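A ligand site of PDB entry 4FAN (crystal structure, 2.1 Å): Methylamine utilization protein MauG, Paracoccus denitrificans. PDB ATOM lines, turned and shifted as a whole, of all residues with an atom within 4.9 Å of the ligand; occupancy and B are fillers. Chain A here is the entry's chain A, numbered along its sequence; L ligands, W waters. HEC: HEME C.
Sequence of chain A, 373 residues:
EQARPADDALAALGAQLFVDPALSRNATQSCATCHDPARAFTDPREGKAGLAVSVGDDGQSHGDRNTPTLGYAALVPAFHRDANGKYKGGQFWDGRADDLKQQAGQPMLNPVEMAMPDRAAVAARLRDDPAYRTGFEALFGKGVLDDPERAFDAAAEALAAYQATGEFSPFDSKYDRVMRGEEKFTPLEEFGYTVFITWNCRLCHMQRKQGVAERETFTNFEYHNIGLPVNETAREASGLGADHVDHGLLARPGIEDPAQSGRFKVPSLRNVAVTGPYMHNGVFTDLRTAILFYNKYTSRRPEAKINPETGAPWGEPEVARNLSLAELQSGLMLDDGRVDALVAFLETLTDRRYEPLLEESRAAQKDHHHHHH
The side-chain amide nitrogen (NE2) of Gln 103 sits close to a nitrogen (NA) of the ligand (3.1 Å). Residues that only touch the ligand: Gln 29 (3.4 Å), Ser 30 (3.6 Å), Ser 54 (3.6 Å), Val 55 (3.6 Å), Asn 66 (3.9 Å), Thr 67 (3.2 Å), Pro 68 (3.3 Å), Leu 70 (3.2 Å), Gln 91 (3.3 Å), Leu 100 (3.3 Å), Ala 104 (3.4 Å), Pro 107 (3.3 Å), Met 108 (3.9 Å), Glu 113 (3.7 Å), Met 114 (3.5 Å) and Gln 163 (3.2 Å). Hydrophobic or aromatic side chains within 4 Å of the ligand: His 35, Pro 68, Leu 70, Phe 92, Trp 93, Leu 100, Pro 107, Met 108 and Met 114. Of the 33 residues printed, 25 come within 4 Å of the ligand. The nearest printed residue that does not touch the ligand is Gly 56 (4.05 Å).
Water W1 lies within hydrogen-bond range of the backbone NH (N) of Ser 54 (2.7 Å) and the backbone carbonyl oxygen (O) of Arg 65 (2.8 Å).
The backbone NH (N) of Cys 31 is in hydrogen-bond range of the backbone carbonyl oxygen (O) of Phe 18, 3.1 Å away. The guanidinium group of Arg 65 lies within salt-bridge range of the side-chain carboxylate of Asp 94 (2.9 Å). OG1 of Thr 67 lies within hydrogen-bond range of OG of Ser 54 (2.5 Å). The side-chain amide oxygen (OE1) of Gln 91 sits close to the backbone carbonyl oxygen (O) of Ala 73, at 3.0 Å. O of Pro 107 is in hydrogen-bond range of N of Met 114 (3.1 Å). The side-chain amide oxygen of Gln 29 sits close to the backbone carbonyl oxygen of Val 55 (2.9 Å). NE2 of Gln 29 sits close to O of Glu 113, at 3.3 Å. The backbone carbonyl oxygen of Val 55 sits at hydrogen-bond distance from the guanidinium group of Arg 45, at 3.1 Å.
The side-chain sulfur (SG) of Cys 31 is covalently linked to a carbon (CAB) of the ligand (1.8 Å). A carbon (CAC) of the ligand is bonded to the side-chain sulfur (SG) of Cys 34, at 1.9 Å. An iron atom (FE) of the ligand is bound by a ring nitrogen (NE2) of His 35 (2.0 Å). NH2 of Arg 96 lies within salt-bridge range of O1D of the ligand. The backbone NH (N) of Phe 92 is in hydrogen-bond range of an oxygen (O2A) of the ligand, at 2.6 Å. NH1 of Arg 65 is in salt-bridge range of O1D of the ligand (3.0 Å). The backbone NH (N) of Trp 93 is in hydrogen-bond range of an oxygen (O2D) of the ligand, at 3.0 Å. The side-chain amino group of Lys 265 is in salt-bridge range of an oxygen (O1A) of the ligand (3.1 Å).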
ATOM      1  N   PHE A  18     -13.587  22.089   2.516  1.00  0.00           N
ATOM      2  CA  PHE A  18     -12.867  23.124   3.156  1.00  0.00           C
ATOM      3  C   PHE A  18     -12.892  22.908   4.664  1.00  0.00           C
ATOM      4  O   PHE A  18     -11.883  23.203   5.333  1.00  0.00           O
ATOM      5  CB  PHE A  18     -13.502  24.449   2.839  1.00  0.00           C
ATOM      6  CG  PHE A  18     -12.746  25.607   3.364  1.00  0.00           C
ATOM      7  CD1 PHE A  18     -11.693  26.142   2.629  1.00  0.00           C
ATOM      8  CD2 PHE A  18     -13.126  26.236   4.563  1.00  0.00           C
ATOM      9  CE1 PHE A  18     -11.027  27.264   3.052  1.00  0.00           C
ATOM     10  CE2 PHE A  18     -12.378  27.353   5.048  1.00  0.00           C
ATOM     11  CZ  PHE A  18     -11.350  27.859   4.274  1.00  0.00           C
ATOM     12  N   GLN A  29      -7.357  18.204  11.295  1.00  0.00           N
ATOM     13  CA  GLN A  29      -7.182  19.554  10.742  1.00  0.00           C
ATOM     14  C   GLN A  29      -7.781  19.715   9.367  1.00  0.00           C
ATOM     15  O   GLN A  29      -7.508  18.898   8.477  1.00  0.00           O
ATOM     16  CB  GLN A  29      -5.709  19.869  10.694  1.00  0.00           C
ATOM     17  CG  GLN A  29      -5.306  21.180  10.016  1.00  0.00           C
ATOM     18  CD  GLN A  29      -3.906  21.588  10.418  1.00  0.00           C
ATOM     19  OE1 GLN A  29      -3.673  22.028  11.572  1.00  0.00           O
ATOM     20  NE2 GLN A  29      -2.967  21.421   9.518  1.00  0.00           N
ATOM     21  N   SER A  30      -8.542  20.779   9.155  1.00  0.00           N
ATOM     22  CA  SER A  30      -9.040  21.088   7.810  1.00  0.00           C
ATOM     23  C   SER A  30      -8.507  22.442   7.382  1.00  0.00           C
ATOM     24  O   SER A  30      -7.831  23.125   8.187  1.00  0.00           O
ATOM     25  CB  SER A  30     -10.548  21.151   7.830  1.00  0.00           C
ATOM     26  OG  SER A  30     -10.950  22.240   8.648  1.00  0.00           O
ATOM     27  N   CYS A  31      -8.870  22.887   6.177  1.00  0.00           N
ATOM     28  CA  CYS A  31      -8.429  24.229   5.745  1.00  0.00           C
ATOM     29  C   CYS A  31      -9.004  25.222   6.748  1.00  0.00           C
ATOM     30  O   CYS A  31      -8.355  26.175   7.089  1.00  0.00           O
ATOM     31  CB  CYS A  31      -8.919  24.648   4.362  1.00  0.00           C
ATOM     32  SG  CYS A  31      -8.988  23.437   3.050  1.00  0.00           S
ATOM     33  N   CYS A  34      -7.066  26.471   9.996  1.00  0.00           N
ATOM     34  CA  CYS A  34      -6.116  27.536   9.901  1.00  0.00           C
ATOM     35  C   CYS A  34      -6.796  28.733   9.275  1.00  0.00           C
ATOM     36  O   CYS A  34      -6.523  29.872   9.656  1.00  0.00           O
ATOM     37  CB  CYS A  34      -4.927  27.121   9.057  1.00  0.00           C
ATOM     38  SG  CYS A  34      -3.851  25.915   9.874  1.00  0.00           S
ATOM     39  N   HIS A  35      -7.627  28.498   8.272  1.00  0.00           N
ATOM     40  CA  HIS A  35      -8.344  29.617   7.679  1.00  0.00           C
ATOM     41  C   HIS A  35      -9.727  29.652   8.332  1.00  0.00           C
ATOM     42  O   HIS A  35     -10.752  29.323   7.738  1.00  0.00           O
ATOM     43  CB  HIS A  35      -8.369  29.530   6.154  1.00  0.00           C
ATOM     44  CG  HIS A  35      -7.000  29.475   5.538  1.00  0.00           C
ATOM     45  ND1 HIS A  35      -6.218  30.595   5.334  1.00  0.00           N
ATOM     46  CD2 HIS A  35      -6.251  28.423   5.125  1.00  0.00           C
ATOM     47  CE1 HIS A  35      -5.076  30.240   4.773  1.00  0.00           C
ATOM     48  NE2 HIS A  35      -5.084  28.929   4.607  1.00  0.00           N
ATOM     49  N   ARG A  45      -5.613  30.206  16.522  1.00  0.00           N
ATOM     50  CA  ARG A  45      -5.074  29.268  17.523  1.00  0.00           C
ATOM     51  C   ARG A  45      -3.696  29.726  18.021  1.00  0.00           C
ATOM     52  O   ARG A  45      -2.833  30.062  17.191  1.00  0.00           O
ATOM     53  CB  ARG A  45      -4.963  27.842  16.946  1.00  0.00           C
ATOM     54  CG  ARG A  45      -6.274  27.016  16.880  1.00  0.00           C
ATOM     55  CD  ARG A  45      -5.986  25.688  16.140  1.00  0.00           C
ATOM     56  NE  ARG A  45      -5.174  25.960  14.932  1.00  0.00           N
ATOM     57  CZ  ARG A  45      -4.352  25.079  14.351  1.00  0.00           C
ATOM     58  NH1 ARG A  45      -4.248  23.808  14.800  1.00  0.00           N
ATOM     59  NH2 ARG A  45      -3.642  25.467  13.285  1.00  0.00           N
ATOM     60  N   SER A  54       1.151  29.155  12.131  1.00  0.00           N
ATOM     61  CA  SER A  54       0.163  28.115  12.438  1.00  0.00           C
ATOM     62  C   SER A  54       0.804  26.744  12.675  1.00  0.00           C
ATOM     63  O   SER A  54       1.913  26.482  12.203  1.00  0.00           O
ATOM     64  CB  SER A  54      -0.819  28.061  11.283  1.00  0.00           C
ATOM     65  OG  SER A  54      -1.567  29.257  11.198  1.00  0.00           O
ATOM     66  N   VAL A  55       0.093  25.871  13.410  1.00  0.00           N
ATOM     67  CA  VAL A  55       0.558  24.518  13.681  1.00  0.00           C
ATOM     68  C   VAL A  55      -0.118  23.478  12.781  1.00  0.00           C
ATOM     69  O   VAL A  55      -1.365  23.437  12.653  1.00  0.00           O
ATOM     70  CB  VAL A  55       0.295  24.149  15.155  1.00  0.00           C
ATOM     71  CG1 VAL A  55       0.852  22.763  15.511  1.00  0.00           C
ATOM     72  CG2 VAL A  55       0.859  25.228  16.050  1.00  0.00           C
ATOM     73  N   GLY A  56       0.699  22.598  12.187  1.00  0.00           N
ATOM     74  CA  GLY A  56       0.149  21.515  11.371  1.00  0.00           C
ATOM     75  C   GLY A  56      -0.646  20.413  12.098  1.00  0.00           C
ATOM     76  O   GLY A  56      -0.759  20.411  13.357  1.00  0.00           O
ATOM     77  N   ARG A  65       5.577  31.262   7.972  1.00  0.00           N
ATOM     78  CA  ARG A  65       4.803  32.423   7.603  1.00  0.00           C
ATOM     79  C   ARG A  65       3.474  32.508   8.313  1.00  0.00           C
ATOM     80  O   ARG A  65       2.932  31.499   8.752  1.00  0.00           O
ATOM     81  CB  ARG A  65       4.594  32.455   6.094  1.00  0.00           C
ATOM     82  CG  ARG A  65       5.918  32.503   5.409  1.00  0.00           C
ATOM     83  CD  ARG A  65       5.728  32.771   4.011  1.00  0.00           C
ATOM     84  NE  ARG A  65       7.042  32.784   3.359  1.00  0.00           N
ATOM     85  CZ  ARG A  65       7.205  32.489   2.090  1.00  0.00           C
ATOM     86  NH1 ARG A  65       6.151  32.197   1.357  1.00  0.00           N
ATOM     87  NH2 ARG A  65       8.399  32.524   1.547  1.00  0.00           N
ATOM     88  N   ASN A  66       2.955  33.735   8.404  1.00  0.00           N
ATOM     89  CA  ASN A  66       1.636  33.994   8.986  1.00  0.00           C
ATOM     90  C   ASN A  66       0.635  33.533   7.946  1.00  0.00           C
ATOM     91  O   ASN A  66       0.842  33.746   6.703  1.00  0.00           O
ATOM     92  CB  ASN A  66       1.488  35.476   9.263  1.00  0.00           C
ATOM     93  CG  ASN A  66       0.148  35.842   9.867  1.00  0.00           C
ATOM     94  OD1 ASN A  66      -0.654  36.594   9.252  1.00  0.00           O
ATOM     95  ND2 ASN A  66      -0.116  35.327  11.080  1.00  0.00           N
ATOM     96  N   THR A  67      -0.401  32.873   8.460  1.00  0.00           N
ATOM     97  CA  THR A  67      -1.507  32.414   7.702  1.00  0.00           C
ATOM     98  C   THR A  67      -2.331  33.604   7.202  1.00  0.00           C
ATOM     99  O   THR A  67      -2.925  34.312   7.992  1.00  0.00           O
ATOM    100  CB  THR A  67      -2.362  31.490   8.590  1.00  0.00           C
ATOM    101  OG1 THR A  67      -1.630  30.293   8.889  1.00  0.00           O
ATOM    102  CG2 THR A  67      -3.742  31.145   7.876  1.00  0.00           C
ATOM    103  N   PRO A  68      -2.371  33.830   5.862  1.00  0.00           N
ATOM    104  CA  PRO A  68      -3.134  34.980   5.422  1.00  0.00           C
ATOM    105  C   PRO A  68      -4.655  34.670   5.296  1.00  0.00           C
ATOM    106  O   PRO A  68      -5.090  33.497   5.134  1.00  0.00           O
ATOM    107  CB  PRO A  68      -2.521  35.292   4.007  1.00  0.00           C
ATOM    108  CG  PRO A  68      -2.206  33.881   3.466  1.00  0.00           C
ATOM    109  CD  PRO A  68      -1.761  33.084   4.742  1.00  0.00           C
ATOM    110  N   THR A  69      -5.472  35.714   5.362  1.00  0.00           N
ATOM    111  CA  THR A  69      -6.916  35.605   5.046  1.00  0.00           C
ATOM    112  C   THR A  69      -7.135  35.019   3.624  1.00  0.00           C
ATOM    113  O   THR A  69      -6.320  35.248   2.726  1.00  0.00           O
ATOM    114  CB  THR A  69      -7.535  36.971   5.011  1.00  0.00           C
ATOM    115  OG1 THR A  69      -8.916  36.817   4.746  1.00  0.00           O
ATOM    116  CG2 THR A  69      -6.864  37.809   3.792  1.00  0.00           C
ATOM    117  N   LEU A  70      -8.218  34.287   3.417  1.00  0.00           N
ATOM    118  CA  LEU A  70      -8.530  33.844   2.064  1.00  0.00           C
ATOM    119  C   LEU A  70      -9.578  34.802   1.443  1.00  0.00           C
ATOM    120  O   LEU A  70      -9.930  34.619   0.289  1.00  0.00           O
ATOM    121  CB  LEU A  70      -9.032  32.391   2.047  1.00  0.00           C
ATOM    122  CG  LEU A  70      -8.188  31.248   2.653  1.00  0.00           C
ATOM    123  CD1 LEU A  70      -8.822  29.915   2.326  1.00  0.00           C
ATOM    124  CD2 LEU A  70      -6.750  31.267   2.186  1.00  0.00           C
ATOM    125  N   ALA A  73      -8.902  36.688  -1.934  1.00  0.00           N
ATOM    126  CA  ALA A  73      -7.780  36.046  -2.620  1.00  0.00           C
ATOM    127  C   ALA A  73      -8.146  35.809  -4.050  1.00  0.00           C
ATOM    128  O   ALA A  73      -7.265  35.786  -4.874  1.00  0.00           O
ATOM    129  CB  ALA A  73      -7.351  34.763  -1.992  1.00  0.00           C
ATOM    130  N   GLN A  91      -0.426  33.306  -5.668  1.00  0.00           N
ATOM    131  CA  GLN A  91      -0.886  33.041  -4.284  1.00  0.00           C
ATOM    132  C   GLN A  91       0.310  32.553  -3.437  1.00  0.00           C
ATOM    133  O   GLN A  91       1.307  32.038  -4.000  1.00  0.00           O
ATOM    134  CB  GLN A  91      -1.983  31.950  -4.262  1.00  0.00           C
ATOM    135  CG  GLN A  91      -3.269  32.303  -5.000  1.00  0.00           C
ATOM    136  CD  GLN A  91      -4.099  33.445  -4.386  1.00  0.00           C
ATOM    137  OE1 GLN A  91      -4.842  34.110  -5.087  1.00  0.00           O
ATOM    138  NE2 GLN A  91      -3.995  33.631  -3.110  1.00  0.00           N
ATOM    139  N   PHE A  92       0.137  32.646  -2.107  1.00  0.00           N
ATOM    140  CA  PHE A  92       1.192  32.581  -1.088  1.00  0.00           C
ATOM    141  C   PHE A  92       1.940  33.907  -1.039  1.00  0.00           C
ATOM    142  O   PHE A  92       1.953  34.662  -2.023  1.00  0.00           O
ATOM    143  CB  PHE A  92       2.255  31.526  -1.372  1.00  0.00           C
ATOM    144  CG  PHE A  92       1.790  30.138  -1.210  1.00  0.00           C
ATOM    145  CD1 PHE A  92       1.204  29.729  -0.025  1.00  0.00           C
ATOM    146  CD2 PHE A  92       1.953  29.231  -2.230  1.00  0.00           C
ATOM    147  CE1 PHE A  92       0.763  28.416   0.156  1.00  0.00           C
ATOM    148  CE2 PHE A  92       1.542  27.918  -2.064  1.00  0.00           C
ATOM    149  CZ  PHE A  92       0.937  27.516  -0.853  1.00  0.00           C
ATOM    150  N   TRP A  93       2.597  34.179   0.077  1.00  0.00           N
ATOM    151  CA  TRP A  93       3.305  35.427   0.256  1.00  0.00           C
ATOM    152  C   TRP A  93       4.440  35.585  -0.736  1.00  0.00           C
ATOM    153  O   TRP A  93       4.885  36.703  -0.997  1.00  0.00           O
ATOM    154  CB  TRP A  93       3.863  35.493   1.636  1.00  0.00           C
ATOM    155  CG  TRP A  93       2.898  35.711   2.728  1.00  0.00           C
ATOM    156  CD1 TRP A  93       2.429  34.749   3.588  1.00  0.00           C
ATOM    157  CD2 TRP A  93       2.371  36.953   3.181  1.00  0.00           C
ATOM    158  NE1 TRP A  93       1.622  35.329   4.524  1.00  0.00           N
ATOM    159  CE2 TRP A  93       1.575  36.678   4.317  1.00  0.00           C
ATOM    160  CE3 TRP A  93       2.505  38.296   2.741  1.00  0.00           C
ATOM    161  CZ2 TRP A  93       0.861  37.696   5.011  1.00  0.00           C
ATOM    162  CZ3 TRP A  93       1.793  39.319   3.466  1.00  0.00           C
ATOM    163  CH2 TRP A  93       1.001  39.003   4.596  1.00  0.00           C
ATOM    164  N   ASP A  94       4.898  34.485  -1.321  1.00  0.00           N
ATOM    165  CA  ASP A  94       6.016  34.551  -2.227  1.00  0.00           C
ATOM    166  C   ASP A  94       5.574  34.293  -3.654  1.00  0.00           C
ATOM    167  O   ASP A  94       6.388  34.091  -4.543  1.00  0.00           O
ATOM    168  CB  ASP A  94       7.154  33.612  -1.790  1.00  0.00           C
ATOM    169  CG  ASP A  94       6.733  32.175  -1.655  1.00  0.00           C
ATOM    170  OD1 ASP A  94       7.527  31.409  -1.070  1.00  0.00           O
ATOM    171  OD2 ASP A  94       5.595  31.831  -2.061  1.00  0.00           O
ATOM    172  N   ARG A  96       4.456  31.827  -5.025  1.00  0.00           N
ATOM    173  CA  ARG A  96       4.984  30.608  -5.594  1.00  0.00           C
ATOM    174  C   ARG A  96       3.901  29.672  -6.203  1.00  0.00           C
ATOM    175  O   ARG A  96       4.235  28.735  -6.939  1.00  0.00           O
ATOM    176  CB  ARG A  96       5.838  29.877  -4.575  1.00  0.00           C
ATOM    177  CG  ARG A  96       5.035  29.289  -3.422  1.00  0.00           C
ATOM    178  CD  ARG A  96       5.911  28.320  -2.614  1.00  0.00           C
ATOM    179  NE  ARG A  96       5.169  27.633  -1.542  1.00  0.00           N
ATOM    180  CZ  ARG A  96       4.836  28.243  -0.392  1.00  0.00           C
ATOM    181  NH1 ARG A  96       4.197  27.582   0.561  1.00  0.00           N
ATOM    182  NH2 ARG A  96       5.171  29.509  -0.186  1.00  0.00           N
ATOM    183  N   LEU A 100      -5.453  30.092  -7.299  1.00  0.00           N
ATOM    184  CA  LEU A 100      -6.089  29.367  -6.181  1.00  0.00           C
ATOM    185  C   LEU A 100      -6.089  27.873  -6.418  1.00  0.00           C
ATOM    186  O   LEU A 100      -5.928  27.084  -5.484  1.00  0.00           O
ATOM    187  CB  LEU A 100      -7.502  29.822  -5.951  1.00  0.00           C
ATOM    188  CG  LEU A 100      -7.543  31.261  -5.430  1.00  0.00           C
ATOM    189  CD1 LEU A 100      -9.035  31.765  -5.440  1.00  0.00           C
ATOM    190  CD2 LEU A 100      -6.896  31.266  -4.053  1.00  0.00           C
ATOM    191  N   GLN A 103      -2.733  26.468  -5.817  1.00  0.00           N
ATOM    192  CA  GLN A 103      -2.464  26.624  -4.387  1.00  0.00           C
ATOM    193  C   GLN A 103      -3.156  25.564  -3.492  1.00  0.00           C
ATOM    194  O   GLN A 103      -2.557  25.116  -2.553  1.00  0.00           O
ATOM    195  CB  GLN A 103      -2.843  28.028  -3.911  1.00  0.00           C
ATOM    196  CG  GLN A 103      -2.414  28.380  -2.435  1.00  0.00           C
ATOM    197  CD  GLN A 103      -3.117  27.550  -1.335  1.00  0.00           C
ATOM    198  OE1 GLN A 103      -4.267  27.136  -1.489  1.00  0.00           O
ATOM    199  NE2 GLN A 103      -2.443  27.340  -0.209  1.00  0.00           N
ATOM    200  N   ALA A 104      -4.387  25.144  -3.812  1.00  0.00           N
ATOM    201  CA  ALA A 104      -5.253  24.356  -2.912  1.00  0.00           C
ATOM    202  C   ALA A 104      -4.706  23.018  -2.435  1.00  0.00           C
ATOM    203  O   ALA A 104      -4.947  22.594  -1.294  1.00  0.00           O
ATOM    204  CB  ALA A 104      -6.663  24.143  -3.573  1.00  0.00           C
ATOM    205  N   PRO A 107      -1.389  22.727   0.828  1.00  0.00           N
ATOM    206  CA  PRO A 107      -1.529  22.449   2.314  1.00  0.00           C
ATOM    207  C   PRO A 107      -1.788  20.998   2.661  1.00  0.00           C
ATOM    208  O   PRO A 107      -1.269  20.511   3.674  1.00  0.00           O
ATOM    209  CB  PRO A 107      -2.713  23.316   2.763  1.00  0.00           C
ATOM    210  CG  PRO A 107      -2.913  24.315   1.603  1.00  0.00           C
ATOM    211  CD  PRO A 107      -2.359  23.742   0.364  1.00  0.00           C
ATOM    212  N   MET A 108      -2.609  20.315   1.848  1.00  0.00           N
ATOM    213  CA  MET A 108      -2.918  18.900   2.040  1.00  0.00           C
ATOM    214  C   MET A 108      -1.717  17.992   2.109  1.00  0.00           C
ATOM    215  O   MET A 108      -1.753  16.957   2.780  1.00  0.00           O
ATOM    216  CB  MET A 108      -3.786  18.352   0.918  1.00  0.00           C
ATOM    217  CG  MET A 108      -5.017  19.156   0.686  1.00  0.00           C
ATOM    218  SD  MET A 108      -6.184  18.252  -0.353  1.00  0.00           S
ATOM    219  CE  MET A 108      -7.034  19.687  -1.003  1.00  0.00           C
ATOM    220  N   VAL A 112       4.227  20.057   7.327  1.00  0.00           N
ATOM    221  CA  VAL A 112       4.124  21.034   8.453  1.00  0.00           C
ATOM    222  C   VAL A 112       2.688  21.572   8.593  1.00  0.00           C
ATOM    223  O   VAL A 112       2.409  22.381   9.485  1.00  0.00           O
ATOM    224  CB  VAL A 112       5.159  22.266   8.366  1.00  0.00           C
ATOM    225  CG1 VAL A 112       6.458  21.894   7.615  1.00  0.00           C
ATOM    226  CG2 VAL A 112       4.529  23.474   7.725  1.00  0.00           C
ATOM    227  N   GLU A 113       1.814  21.135   7.667  1.00  0.00           N
ATOM    228  CA  GLU A 113       0.396  21.503   7.669  1.00  0.00           C
ATOM    229  C   GLU A 113      -0.466  20.225   7.753  1.00  0.00           C
ATOM    230  O   GLU A 113      -0.400  19.502   8.740  1.00  0.00           O
ATOM    231  CB  GLU A 113       0.035  22.460   6.480  1.00  0.00           C
ATOM    232  CG  GLU A 113       0.831  23.828   6.534  1.00  0.00           C
ATOM    233  CD  GLU A 113       0.633  24.778   5.272  1.00  0.00           C
ATOM    234  OE1 GLU A 113      -0.047  24.442   4.294  1.00  0.00           O
ATOM    235  OE2 GLU A 113       1.168  25.909   5.285  1.00  0.00           O
ATOM    236  N   MET A 114      -1.253  19.931   6.737  1.00  0.00           N
ATOM    237  CA  MET A 114      -2.202  18.826   6.772  1.00  0.00           C
ATOM    238  C   MET A 114      -1.583  17.446   6.639  1.00  0.00           C
ATOM    239  O   MET A 114      -2.179  16.448   7.074  1.00  0.00           O
ATOM    240  CB  MET A 114      -3.340  19.069   5.790  1.00  0.00           C
ATOM    241  CG  MET A 114      -4.063  20.356   6.067  1.00  0.00           C
ATOM    242  SD  MET A 114      -5.224  20.825   4.758  1.00  0.00           S
ATOM    243  CE  MET A 114      -6.606  19.770   5.154  1.00  0.00           C
ATOM    244  N   LEU A 159     -12.217  23.498  -4.051  1.00  0.00           N
ATOM    245  CA  LEU A 159     -11.739  24.522  -3.119  1.00  0.00           C
ATOM    246  C   LEU A 159     -11.559  25.915  -3.741  1.00  0.00           C
ATOM    247  O   LEU A 159     -11.994  26.941  -3.136  1.00  0.00           O
ATOM    248  CB  LEU A 159     -10.468  24.052  -2.449  1.00  0.00           C
ATOM    249  CG  LEU A 159     -10.835  22.827  -1.558  1.00  0.00           C
ATOM    250  CD1 LEU A 159      -9.545  22.020  -1.323  1.00  0.00           C
ATOM    251  CD2 LEU A 159     -11.447  23.264  -0.171  1.00  0.00           C
ATOM    252  N   GLN A 163     -13.594  29.233  -2.768  1.00  0.00           N
ATOM    253  CA  GLN A 163     -12.997  30.559  -2.479  1.00  0.00           C
ATOM    254  C   GLN A 163     -13.325  31.720  -3.432  1.00  0.00           C
ATOM    255  O   GLN A 163     -13.019  32.888  -3.088  1.00  0.00           O
ATOM    256  CB  GLN A 163     -11.475  30.531  -2.248  1.00  0.00           C
ATOM    257  CG  GLN A 163     -11.000  29.566  -1.132  1.00  0.00           C
ATOM    258  CD  GLN A 163      -9.547  29.210  -1.347  1.00  0.00           C
ATOM    259  OE1 GLN A 163      -9.225  28.252  -2.055  1.00  0.00           O
ATOM    260  NE2 GLN A 163      -8.659  30.019  -0.807  1.00  0.00           N
ATOM    261  N   LYS A 265       4.356  39.543  -1.735  1.00  0.00           N
ATOM    262  CA  LYS A 265       3.150  40.054  -2.353  1.00  0.00           C
ATOM    263  C   LYS A 265       2.504  41.103  -1.483  1.00  0.00           C
ATOM    264  O   LYS A 265       2.401  40.905  -0.291  1.00  0.00           O
ATOM    265  CB  LYS A 265       2.154  38.918  -2.544  1.00  0.00           C
ATOM    266  CG  LYS A 265       0.827  39.371  -3.132  1.00  0.00           C
ATOM    267  CD  LYS A 265       0.089  38.216  -3.752  1.00  0.00           C
ATOM    268  CE  LYS A 265      -0.295  37.084  -2.779  1.00  0.00           C
ATOM    269  NZ  LYS A 265      -0.973  37.436  -1.472  1.00  0.00           N
HETATM  270 FE   HEC L   1      -3.675  27.913   3.651  1.00  0.00          FE
HETATM  271  CHA HEC L   1      -1.778  30.408   2.292  1.00  0.00           C
HETATM  272  CHB HEC L   1      -5.813  28.154   0.992  1.00  0.00           C
HETATM  273  CHC HEC L   1      -5.014  24.907   4.586  1.00  0.00           C
HETATM  274  CHD HEC L   1      -1.971  28.120   6.567  1.00  0.00           C
HETATM  275  NA  HEC L   1      -3.798  29.084   1.910  1.00  0.00           N
HETATM  276  C1A HEC L   1      -2.986  30.069   1.533  1.00  0.00           C
HETATM  277  C2A HEC L   1      -3.413  30.791   0.311  1.00  0.00           C
HETATM  278  C3A HEC L   1      -4.550  30.130  -0.074  1.00  0.00           C
HETATM  279  C4A HEC L   1      -4.713  29.082   0.966  1.00  0.00           C
HETATM  280  CMA HEC L   1      -5.495  30.348  -1.225  1.00  0.00           C
HETATM  281  CAA HEC L   1      -2.711  31.983  -0.306  1.00  0.00           C
HETATM  282  CBA HEC L   1      -3.370  33.239   0.245  1.00  0.00           C
HETATM  283  CGA HEC L   1      -2.526  34.449  -0.241  1.00  0.00           C
HETATM  284  O1A HEC L   1      -2.985  35.573  -0.089  1.00  0.00           O
HETATM  285  O2A HEC L   1      -1.373  34.333  -0.758  1.00  0.00           O
HETATM  286  NB  HEC L   1      -5.191  26.749   2.953  1.00  0.00           N
HETATM  287  C1B HEC L   1      -5.889  26.936   1.820  1.00  0.00           C
HETATM  288  C2B HEC L   1      -6.803  25.822   1.496  1.00  0.00           C
HETATM  289  C3B HEC L   1      -6.583  24.872   2.502  1.00  0.00           C
HETATM  290  C4B HEC L   1      -5.571  25.523   3.376  1.00  0.00           C
HETATM  291  CMB HEC L   1      -7.687  25.750   0.292  1.00  0.00           C
HETATM  292  CAB HEC L   1      -7.220  23.540   2.652  1.00  0.00           C
HETATM  293  CBB HEC L   1      -6.729  22.584   1.607  1.00  0.00           C
HETATM  294  NC  HEC L   1      -3.513  26.727   5.341  1.00  0.00           N
HETATM  295  C1C HEC L   1      -4.112  25.544   5.551  1.00  0.00           C
HETATM  296  C2C HEC L   1      -3.817  24.933   6.858  1.00  0.00           C
HETATM  297  C3C HEC L   1      -2.936  25.826   7.475  1.00  0.00           C
HETATM  298  C4C HEC L   1      -2.777  26.890   6.438  1.00  0.00           C
HETATM  299  CMC HEC L   1      -4.407  23.626   7.312  1.00  0.00           C
HETATM  300  CAC HEC L   1      -2.284  25.777   8.851  1.00  0.00           C
HETATM  301  CBC HEC L   1      -1.585  24.488   9.243  1.00  0.00           C
HETATM  302  ND  HEC L   1      -2.139  29.116   4.360  1.00  0.00           N
HETATM  303  C1D HEC L   1      -1.444  28.951   5.473  1.00  0.00           C
HETATM  304  C2D HEC L   1      -0.143  29.678   5.509  1.00  0.00           C
HETATM  305  C3D HEC L   1      -0.087  30.309   4.276  1.00  0.00           C
HETATM  306  C4D HEC L   1      -1.356  29.927   3.630  1.00  0.00           C
HETATM  307  CMD HEC L   1       0.907  29.694   6.594  1.00  0.00           C
HETATM  308  CAD HEC L   1       1.024  31.185   3.740  1.00  0.00           C
HETATM  309  CBD HEC L   1       2.020  30.202   3.134  1.00  0.00           C
HETATM  310  CGD HEC L   1       3.177  30.844   2.422  1.00  0.00           C
HETATM  311  O1D HEC L   1       4.181  30.122   2.166  1.00  0.00           O
HETATM  312  O2D HEC L   1       3.089  32.048   2.109  1.00  0.00           O
HETATM  313  O   HOH W   1       2.086  28.903   9.569  1.00  0.00           O
HETATM  314  O   HOH W   2      -6.653  27.535  -2.932  1.00  0.00           O
HETATM  315  O   HOH W   3      -0.246  26.921   3.202  1.00  0.00           O
